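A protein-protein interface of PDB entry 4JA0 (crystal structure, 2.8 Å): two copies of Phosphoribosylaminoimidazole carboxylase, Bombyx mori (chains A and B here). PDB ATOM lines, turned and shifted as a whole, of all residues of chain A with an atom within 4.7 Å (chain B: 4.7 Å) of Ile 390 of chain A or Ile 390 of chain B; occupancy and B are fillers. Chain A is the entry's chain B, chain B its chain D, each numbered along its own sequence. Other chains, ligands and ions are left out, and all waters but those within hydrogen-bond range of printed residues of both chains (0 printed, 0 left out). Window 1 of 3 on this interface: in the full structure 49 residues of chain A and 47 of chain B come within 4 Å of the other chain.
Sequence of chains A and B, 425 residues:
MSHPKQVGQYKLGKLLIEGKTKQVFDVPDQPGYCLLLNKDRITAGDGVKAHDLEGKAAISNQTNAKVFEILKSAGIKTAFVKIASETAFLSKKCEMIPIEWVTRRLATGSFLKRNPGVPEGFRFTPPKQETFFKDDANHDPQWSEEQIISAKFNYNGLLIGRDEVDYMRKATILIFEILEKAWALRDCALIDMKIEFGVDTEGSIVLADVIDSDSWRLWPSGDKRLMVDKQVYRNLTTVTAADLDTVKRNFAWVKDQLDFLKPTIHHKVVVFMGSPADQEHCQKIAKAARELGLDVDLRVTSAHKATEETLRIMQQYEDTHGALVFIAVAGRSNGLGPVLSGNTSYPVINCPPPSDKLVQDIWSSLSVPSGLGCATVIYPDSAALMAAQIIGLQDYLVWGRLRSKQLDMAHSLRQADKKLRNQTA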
ATOM      1  N   VAL A 325     -11.641  -3.001  27.711  1.00  0.00           N
ATOM      2  CA  VAL A 325     -10.877  -1.919  28.316  1.00  0.00           C
ATOM      3  C   VAL A 325     -10.732  -2.155  29.804  1.00  0.00           C
ATOM      4  O   VAL A 325     -11.714  -2.389  30.520  1.00  0.00           O
ATOM      5  CB  VAL A 325     -11.513  -0.520  28.064  1.00  0.00           C
ATOM      6  CG1 VAL A 325     -10.848   0.534  28.926  1.00  0.00           C
ATOM      7  CG2 VAL A 325     -11.384  -0.147  26.609  1.00  0.00           C
ATOM      8  N   PRO A 347      -5.940  -1.967  25.933  1.00  0.00           N
ATOM      9  CA  PRO A 347      -5.715  -0.671  26.585  1.00  0.00           C
ATOM     10  C   PRO A 347      -6.014  -0.681  28.082  1.00  0.00           C
ATOM     11  O   PRO A 347      -7.024  -1.246  28.518  1.00  0.00           O
ATOM     12  CB  PRO A 347      -6.700   0.265  25.862  1.00  0.00           C
ATOM     13  CG  PRO A 347      -7.668  -0.644  25.167  1.00  0.00           C
ATOM     14  CD  PRO A 347      -6.887  -1.852  24.812  1.00  0.00           C
ATOM     15  N   ILE A 349      -6.308   1.967  31.454  1.00  0.00           N
ATOM     16  CA  ILE A 349      -6.361   3.338  31.938  1.00  0.00           C
ATOM     17  C   ILE A 349      -6.167   3.372  33.442  1.00  0.00           C
ATOM     18  O   ILE A 349      -6.757   2.556  34.172  1.00  0.00           O
ATOM     19  CB  ILE A 349      -7.706   4.040  31.630  1.00  0.00           C
ATOM     20  CG1 ILE A 349      -8.106   3.842  30.173  1.00  0.00           C
ATOM     21  CG2 ILE A 349      -7.625   5.518  31.946  1.00  0.00           C
ATOM     22  CD1 ILE A 349      -9.534   4.264  29.902  1.00  0.00           C
ATOM     23  N   MET A 386     -12.957   8.141  28.410  1.00  0.00           N
ATOM     24  CA  MET A 386     -11.877   7.513  27.642  1.00  0.00           C
ATOM     25  C   MET A 386     -12.306   6.119  27.224  1.00  0.00           C
ATOM     26  O   MET A 386     -12.118   5.722  26.070  1.00  0.00           O
ATOM     27  CB  MET A 386     -10.597   7.386  28.464  1.00  0.00           C
ATOM     28  CG  MET A 386      -9.454   8.251  27.991  1.00  0.00           C
ATOM     29  SD  MET A 386      -8.955   8.112  26.257  1.00  0.00           S
ATOM     30  CE  MET A 386      -8.044   6.576  26.396  1.00  0.00           C
ATOM     31  N   ALA A 387     -12.880   5.380  28.171  1.00  0.00           N
ATOM     32  CA  ALA A 387     -13.339   4.033  27.898  1.00  0.00           C
ATOM     33  C   ALA A 387     -14.372   4.080  26.795  1.00  0.00           C
ATOM     34  O   ALA A 387     -14.244   3.357  25.815  1.00  0.00           O
ATOM     35  CB  ALA A 387     -13.918   3.405  29.143  1.00  0.00           C
ATOM     36  N   ALA A 388     -15.354   4.975  26.919  1.00  0.00           N
ATOM     37  CA  ALA A 388     -16.394   5.133  25.885  1.00  0.00           C
ATOM     38  C   ALA A 388     -15.845   5.615  24.554  1.00  0.00           C
ATOM     39  O   ALA A 388     -16.303   5.192  23.512  1.00  0.00           O
ATOM     40  CB  ALA A 388     -17.519   6.046  26.363  1.00  0.00           C
ATOM     41  N   GLN A 389     -14.890   6.530  24.587  1.00  0.00           N
ATOM     42  CA  GLN A 389     -14.321   7.006  23.333  1.00  0.00           C
ATOM     43  C   GLN A 389     -13.629   5.866  22.585  1.00  0.00           C
ATOM     44  O   GLN A 389     -13.639   5.814  21.363  1.00  0.00           O
ATOM     45  CB  GLN A 389     -13.357   8.171  23.573  1.00  0.00           C
ATOM     46  CG  GLN A 389     -14.083   9.440  23.935  1.00  0.00           C
ATOM     47  CD  GLN A 389     -13.166  10.514  24.474  1.00  0.00           C
ATOM     48  OE1 GLN A 389     -12.012  10.248  24.832  1.00  0.00           O
ATOM     49  NE2 GLN A 389     -13.677  11.741  24.549  1.00  0.00           N
ATOM     50  N   ILE A 390     -13.072   4.922  23.322  1.00  0.00           N
ATOM     51  CA  ILE A 390     -12.395   3.807  22.698  1.00  0.00           C
ATOM     52  C   ILE A 390     -13.432   2.867  22.104  1.00  0.00           C
ATOM     53  O   ILE A 390     -13.373   2.531  20.926  1.00  0.00           O
ATOM     54  CB  ILE A 390     -11.516   3.076  23.720  1.00  0.00           C
ATOM     55  CG1 ILE A 390     -10.366   4.003  24.155  1.00  0.00           C
ATOM     56  CG2 ILE A 390     -11.012   1.763  23.132  1.00  0.00           C
ATOM     57  CD1 ILE A 390      -9.589   3.536  25.359  1.00  0.00           C
ATOM     58  N   ILE A 391     -14.422   2.518  22.913  1.00  0.00           N
ATOM     59  CA  ILE A 391     -15.479   1.608  22.510  1.00  0.00           C
ATOM     60  C   ILE A 391     -16.390   2.147  21.389  1.00  0.00           C
ATOM     61  O   ILE A 391     -16.847   1.390  20.521  1.00  0.00           O
ATOM     62  CB  ILE A 391     -16.301   1.225  23.748  1.00  0.00           C
ATOM     63  CG1 ILE A 391     -15.527   0.196  24.557  1.00  0.00           C
ATOM     64  CG2 ILE A 391     -17.622   0.620  23.383  1.00  0.00           C
ATOM     65  CD1 ILE A 391     -16.240  -0.205  25.802  1.00  0.00           C
ATOM     66  N   GLY A 392     -16.594   3.460  21.368  1.00  0.00           N
ATOM     67  CA  GLY A 392     -17.371   4.087  20.325  1.00  0.00           C
ATOM     68  C   GLY A 392     -16.768   3.942  18.938  1.00  0.00           C
ATOM     69  O   GLY A 392     -17.459   4.188  17.942  1.00  0.00           O
ATOM     70  N   LEU A 393     -15.501   3.535  18.844  1.00  0.00           N
ATOM     71  CA  LEU A 393     -14.906   3.329  17.528  1.00  0.00           C
ATOM     72  C   LEU A 393     -15.556   2.125  16.859  1.00  0.00           C
ATOM     73  O   LEU A 393     -15.465   1.965  15.640  1.00  0.00           O
ATOM     74  CB  LEU A 393     -13.394   3.128  17.610  1.00  0.00           C
ATOM     75  CG  LEU A 393     -12.583   4.334  18.063  1.00  0.00           C
ATOM     76  CD1 LEU A 393     -11.087   4.102  17.938  1.00  0.00           C
ATOM     77  CD2 LEU A 393     -13.021   5.549  17.278  1.00  0.00           C
ATOM     78  N   GLN A 394     -16.244   1.317  17.673  1.00  0.00           N
ATOM     79  CA  GLN A 394     -16.909   0.084  17.240  1.00  0.00           C
ATOM     80  C   GLN A 394     -18.419   0.081  17.492  1.00  0.00           C
ATOM     81  O   GLN A 394     -19.135  -0.811  17.047  1.00  0.00           O
ATOM     82  CB  GLN A 394     -16.285  -1.090  17.958  1.00  0.00           C
ATOM     83  CG  GLN A 394     -15.109  -1.666  17.226  1.00  0.00           C
ATOM     84  CD  GLN A 394     -14.290  -2.562  18.111  1.00  0.00           C
ATOM     85  OE1 GLN A 394     -14.239  -2.356  19.318  1.00  0.00           O
ATOM     86  NE2 GLN A 394     -13.664  -3.575  17.528  1.00  0.00           N
ATOM     87  N   VAL B 325      -7.629   8.029  15.939  1.00  0.00           N
ATOM     88  CA  VAL B 325      -7.053   8.420  17.223  1.00  0.00           C
ATOM     89  C   VAL B 325      -6.245   9.701  17.080  1.00  0.00           C
ATOM     90  O   VAL B 325      -5.443   9.825  16.155  1.00  0.00           O
ATOM     91  CB  VAL B 325      -6.152   7.326  17.809  1.00  0.00           C
ATOM     92  CG1 VAL B 325      -5.415   7.864  19.022  1.00  0.00           C
ATOM     93  CG2 VAL B 325      -6.977   6.160  18.198  1.00  0.00           C
ATOM     94  N   PRO B 347     -11.018   9.367  20.769  1.00  0.00           N
ATOM     95  CA  PRO B 347     -10.001   9.415  21.834  1.00  0.00           C
ATOM     96  C   PRO B 347      -8.850  10.375  21.567  1.00  0.00           C
ATOM     97  O   PRO B 347      -8.246  10.388  20.501  1.00  0.00           O
ATOM     98  CB  PRO B 347      -9.472   7.968  21.891  1.00  0.00           C
ATOM     99  CG  PRO B 347      -9.926   7.324  20.625  1.00  0.00           C
ATOM    100  CD  PRO B 347     -11.235   7.989  20.291  1.00  0.00           C
ATOM    101  N   ILE B 349      -5.146  11.518  23.160  1.00  0.00           N
ATOM    102  CA  ILE B 349      -4.065  11.233  24.111  1.00  0.00           C
ATOM    103  C   ILE B 349      -3.057  12.344  24.137  1.00  0.00           C
ATOM    104  O   ILE B 349      -2.525  12.729  23.083  1.00  0.00           O
ATOM    105  CB  ILE B 349      -3.298   9.963  23.761  1.00  0.00           C
ATOM    106  CG1 ILE B 349      -4.260   8.829  23.424  1.00  0.00           C
ATOM    107  CG2 ILE B 349      -2.383   9.588  24.916  1.00  0.00           C
ATOM    108  CD1 ILE B 349      -3.568   7.683  22.766  1.00  0.00           C
ATOM    109  N   MET B 386      -0.450   3.185  23.233  1.00  0.00           N
ATOM    110  CA  MET B 386      -1.846   3.460  23.597  1.00  0.00           C
ATOM    111  C   MET B 386      -2.749   3.495  22.383  1.00  0.00           C
ATOM    112  O   MET B 386      -3.836   2.919  22.415  1.00  0.00           O
ATOM    113  CB  MET B 386      -1.987   4.793  24.318  1.00  0.00           C
ATOM    114  CG  MET B 386      -2.422   4.666  25.747  1.00  0.00           C
ATOM    115  SD  MET B 386      -3.918   3.689  25.998  1.00  0.00           S
ATOM    116  CE  MET B 386      -5.124   4.890  25.463  1.00  0.00           C
ATOM    117  N   ALA B 387      -2.301   4.192  21.338  1.00  0.00           N
ATOM    118  CA  ALA B 387      -3.040   4.292  20.083  1.00  0.00           C
ATOM    119  C   ALA B 387      -3.217   2.917  19.443  1.00  0.00           C
ATOM    120  O   ALA B 387      -4.313   2.544  19.012  1.00  0.00           O
ATOM    121  CB  ALA B 387      -2.314   5.242  19.121  1.00  0.00           C
ATOM    122  N   ALA B 388      -2.122   2.172  19.393  1.00  0.00           N
ATOM    123  CA  ALA B 388      -2.118   0.816  18.883  1.00  0.00           C
ATOM    124  C   ALA B 388      -3.021  -0.111  19.704  1.00  0.00           C
ATOM    125  O   ALA B 388      -3.712  -0.968  19.144  1.00  0.00           O
ATOM    126  CB  ALA B 388      -0.694   0.282  18.831  1.00  0.00           C
ATOM    127  N   GLN B 389      -2.999   0.026  21.025  1.00  0.00           N
ATOM    128  CA  GLN B 389      -3.875  -0.796  21.845  1.00  0.00           C
ATOM    129  C   GLN B 389      -5.334  -0.503  21.569  1.00  0.00           C
ATOM    130  O   GLN B 389      -6.175  -1.391  21.668  1.00  0.00           O
ATOM    131  CB  GLN B 389      -3.577  -0.628  23.330  1.00  0.00           C
ATOM    132  CG  GLN B 389      -2.362  -1.367  23.791  1.00  0.00           C
ATOM    133  CD  GLN B 389      -1.908  -0.879  25.144  1.00  0.00           C
ATOM    134  OE1 GLN B 389      -2.268   0.227  25.572  1.00  0.00           O
ATOM    135  NE2 GLN B 389      -1.158  -1.720  25.859  1.00  0.00           N
ATOM    136  N   ILE B 390      -5.635   0.737  21.208  1.00  0.00           N
ATOM    137  CA  ILE B 390      -7.012   1.130  20.894  1.00  0.00           C
ATOM    138  C   ILE B 390      -7.433   0.551  19.551  1.00  0.00           C
ATOM    139  O   ILE B 390      -8.443  -0.155  19.461  1.00  0.00           O
ATOM    140  CB  ILE B 390      -7.161   2.665  20.860  1.00  0.00           C
ATOM    141  CG1 ILE B 390      -7.117   3.217  22.284  1.00  0.00           C
ATOM    142  CG2 ILE B 390      -8.474   3.046  20.217  1.00  0.00           C
ATOM    143  CD1 ILE B 390      -7.001   4.679  22.365  1.00  0.00           C
ATOM    144  N   ILE B 391      -6.599   0.796  18.540  1.00  0.00           N
ATOM    145  CA  ILE B 391      -6.803   0.320  17.178  1.00  0.00           C
ATOM    146  C   ILE B 391      -6.687  -1.223  17.091  1.00  0.00           C
ATOM    147  O   ILE B 391      -7.315  -1.884  16.246  1.00  0.00           O
ATOM    148  CB  ILE B 391      -5.795   1.005  16.262  1.00  0.00           C
ATOM    149  CG1 ILE B 391      -6.104   2.487  16.188  1.00  0.00           C
ATOM    150  CG2 ILE B 391      -5.787   0.391  14.890  1.00  0.00           C
ATOM    151  CD1 ILE B 391      -5.109   3.228  15.384  1.00  0.00           C
ATOM    152  N   GLY B 392      -5.887  -1.789  17.987  1.00  0.00           N
ATOM    153  CA  GLY B 392      -5.744  -3.219  18.080  1.00  0.00           C
ATOM    154  C   GLY B 392      -7.048  -3.895  18.446  1.00  0.00           C
ATOM    155  O   GLY B 392      -7.179  -5.110  18.301  1.00  0.00           O
ATOM    156  N   LEU B 393      -8.018  -3.126  18.915  1.00  0.00           N
ATOM    157  CA  LEU B 393      -9.332  -3.689  19.188  1.00  0.00           C
ATOM    158  C   LEU B 393     -10.090  -4.058  17.912  1.00  0.00           C
ATOM    159  O   LEU B 393     -11.102  -4.751  17.972  1.00  0.00           O
ATOM    160  CB  LEU B 393     -10.164  -2.727  20.029  1.00  0.00           C
ATOM    161  CG  LEU B 393      -9.664  -2.570  21.463  1.00  0.00           C
ATOM    162  CD1 LEU B 393     -10.584  -1.664  22.236  1.00  0.00           C
ATOM    163  CD2 LEU B 393      -9.568  -3.931  22.123  1.00  0.00           C
ATOM    164  N   GLN B 394      -9.609  -3.574  16.769  1.00  0.00           N
ATOM    165  CA  GLN B 394     -10.260  -3.803  15.478  1.00  0.00           C
ATOM    166  C   GLN B 394      -9.353  -4.494  14.476  1.00  0.00           C
ATOM    167  O   GLN B 394      -9.800  -4.916  13.400  1.00  0.00           O
ATOM    168  CB  GLN B 394     -10.691  -2.476  14.859  1.00  0.00           C
ATOM    169  CG  GLN B 394     -12.052  -2.022  15.259  1.00  0.00           C
ATOM    170  CD  GLN B 394     -12.309  -0.618  14.811  1.00  0.00           C
ATOM    171  OE1 GLN B 394     -11.378   0.159  14.660  1.00  0.00           O
ATOM    172  NE2 GLN B 394     -13.570  -0.282  14.585  1.00  0.00           N
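The backbone carbonyl oxygen of Leu 393 of chain A sits at hydrogen-bond distance from the side-chain amide nitrogen of Gln 394 of chain B (3.1 Å). The side-chain amide nitrogen (NE2) of Gln 394 of chain A is in hydrogen-bond range of the backbone carbonyl oxygen (O) of Leu 393 of chain B.
O of Gln 389 of chain B touches CD of Pro 347 of chain A, 3.3 Å away. CE of Met 386 of chain B touches CE of Met 386 of chain A, at 3.5 Å. CD of Pro 347 of chain B touches O of Gln 389 of chain A, 3.4 Å away. Ile 390 of chain A touches Ile 390 of chain B. Ile 390 of chain A touches Leu 393 of chain B (CG2 to CD1, 3.6 Å). CD1 of Leu 393 of chain A touches CG2 of Ile 390 of chain B (3.6 Å). CG of Gln 394 of chain B touches NE2 of Gln 394 of chain A (3.2 Å).
Of chain B, only Ile 390 (3.8 Å) and Leu 393 (3.6 Å) come within 4 Å of Ile 390 of chain A. Ile 390 of chain B touches just these residues of chain A: Ile 390 and Leu 393. Printed residues of chain A within 4 Å of Pro 347 of chain B: Gln 389. Of the printed residues of chain A, Gln 394 of chain B touches Leu 393 and Gln 394. Printed residues of chain A within 4 Å of Leu 393 of chain B: Ile 390 (3.6 Å) and Gln 394 (2.9 Å). Printed residues of chain A within 4 Å of Gln 389 of chain B: Pro 347. The nearest printed residue of chain B that does not touch Ile 390 of chain A is Pro 347 of chain B (4.7 Å). The nearest residue of chain A that does not touch Ile 390 of chain B is Met 386 of chain A (4.6 Å).
Hydrophobic or aromatic side chains of chain A within 4 Å of the printed part of chain B: Pro 347, Met 386, Ile 390 and Leu 393. Of the 12 printed residues of chain B, 6 touch a printed residue of chain A. Among the printed residues, no Asp or Glu carboxylate lies within 4 Å of a Lys or Arg side-chain nitrogen of the other chain.
Pro 347 of chain A touches Gln 389 of chain B, and with the chains exchanged Gln 389 of chain A touches Pro 347 of chain B. Met 386 of chain A touches its own counterpart, Met 386 of chain B. Leu 393 of chain A touches Gln 394 of chain B, and with the chains exchanged Gln 394 of chain A touches Leu 393 of chain B. Gln 394 of chain A touches its own counterpart, Gln 394 of chain B. Positions printed for both chains: 325, 347, 349, 386, 387, 388, 389, 390, 391, 392, 393 and 394. Of the 9 pairs that touch across the chains among the printed residues, 9 have their exchanged pair printed and touching as well.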
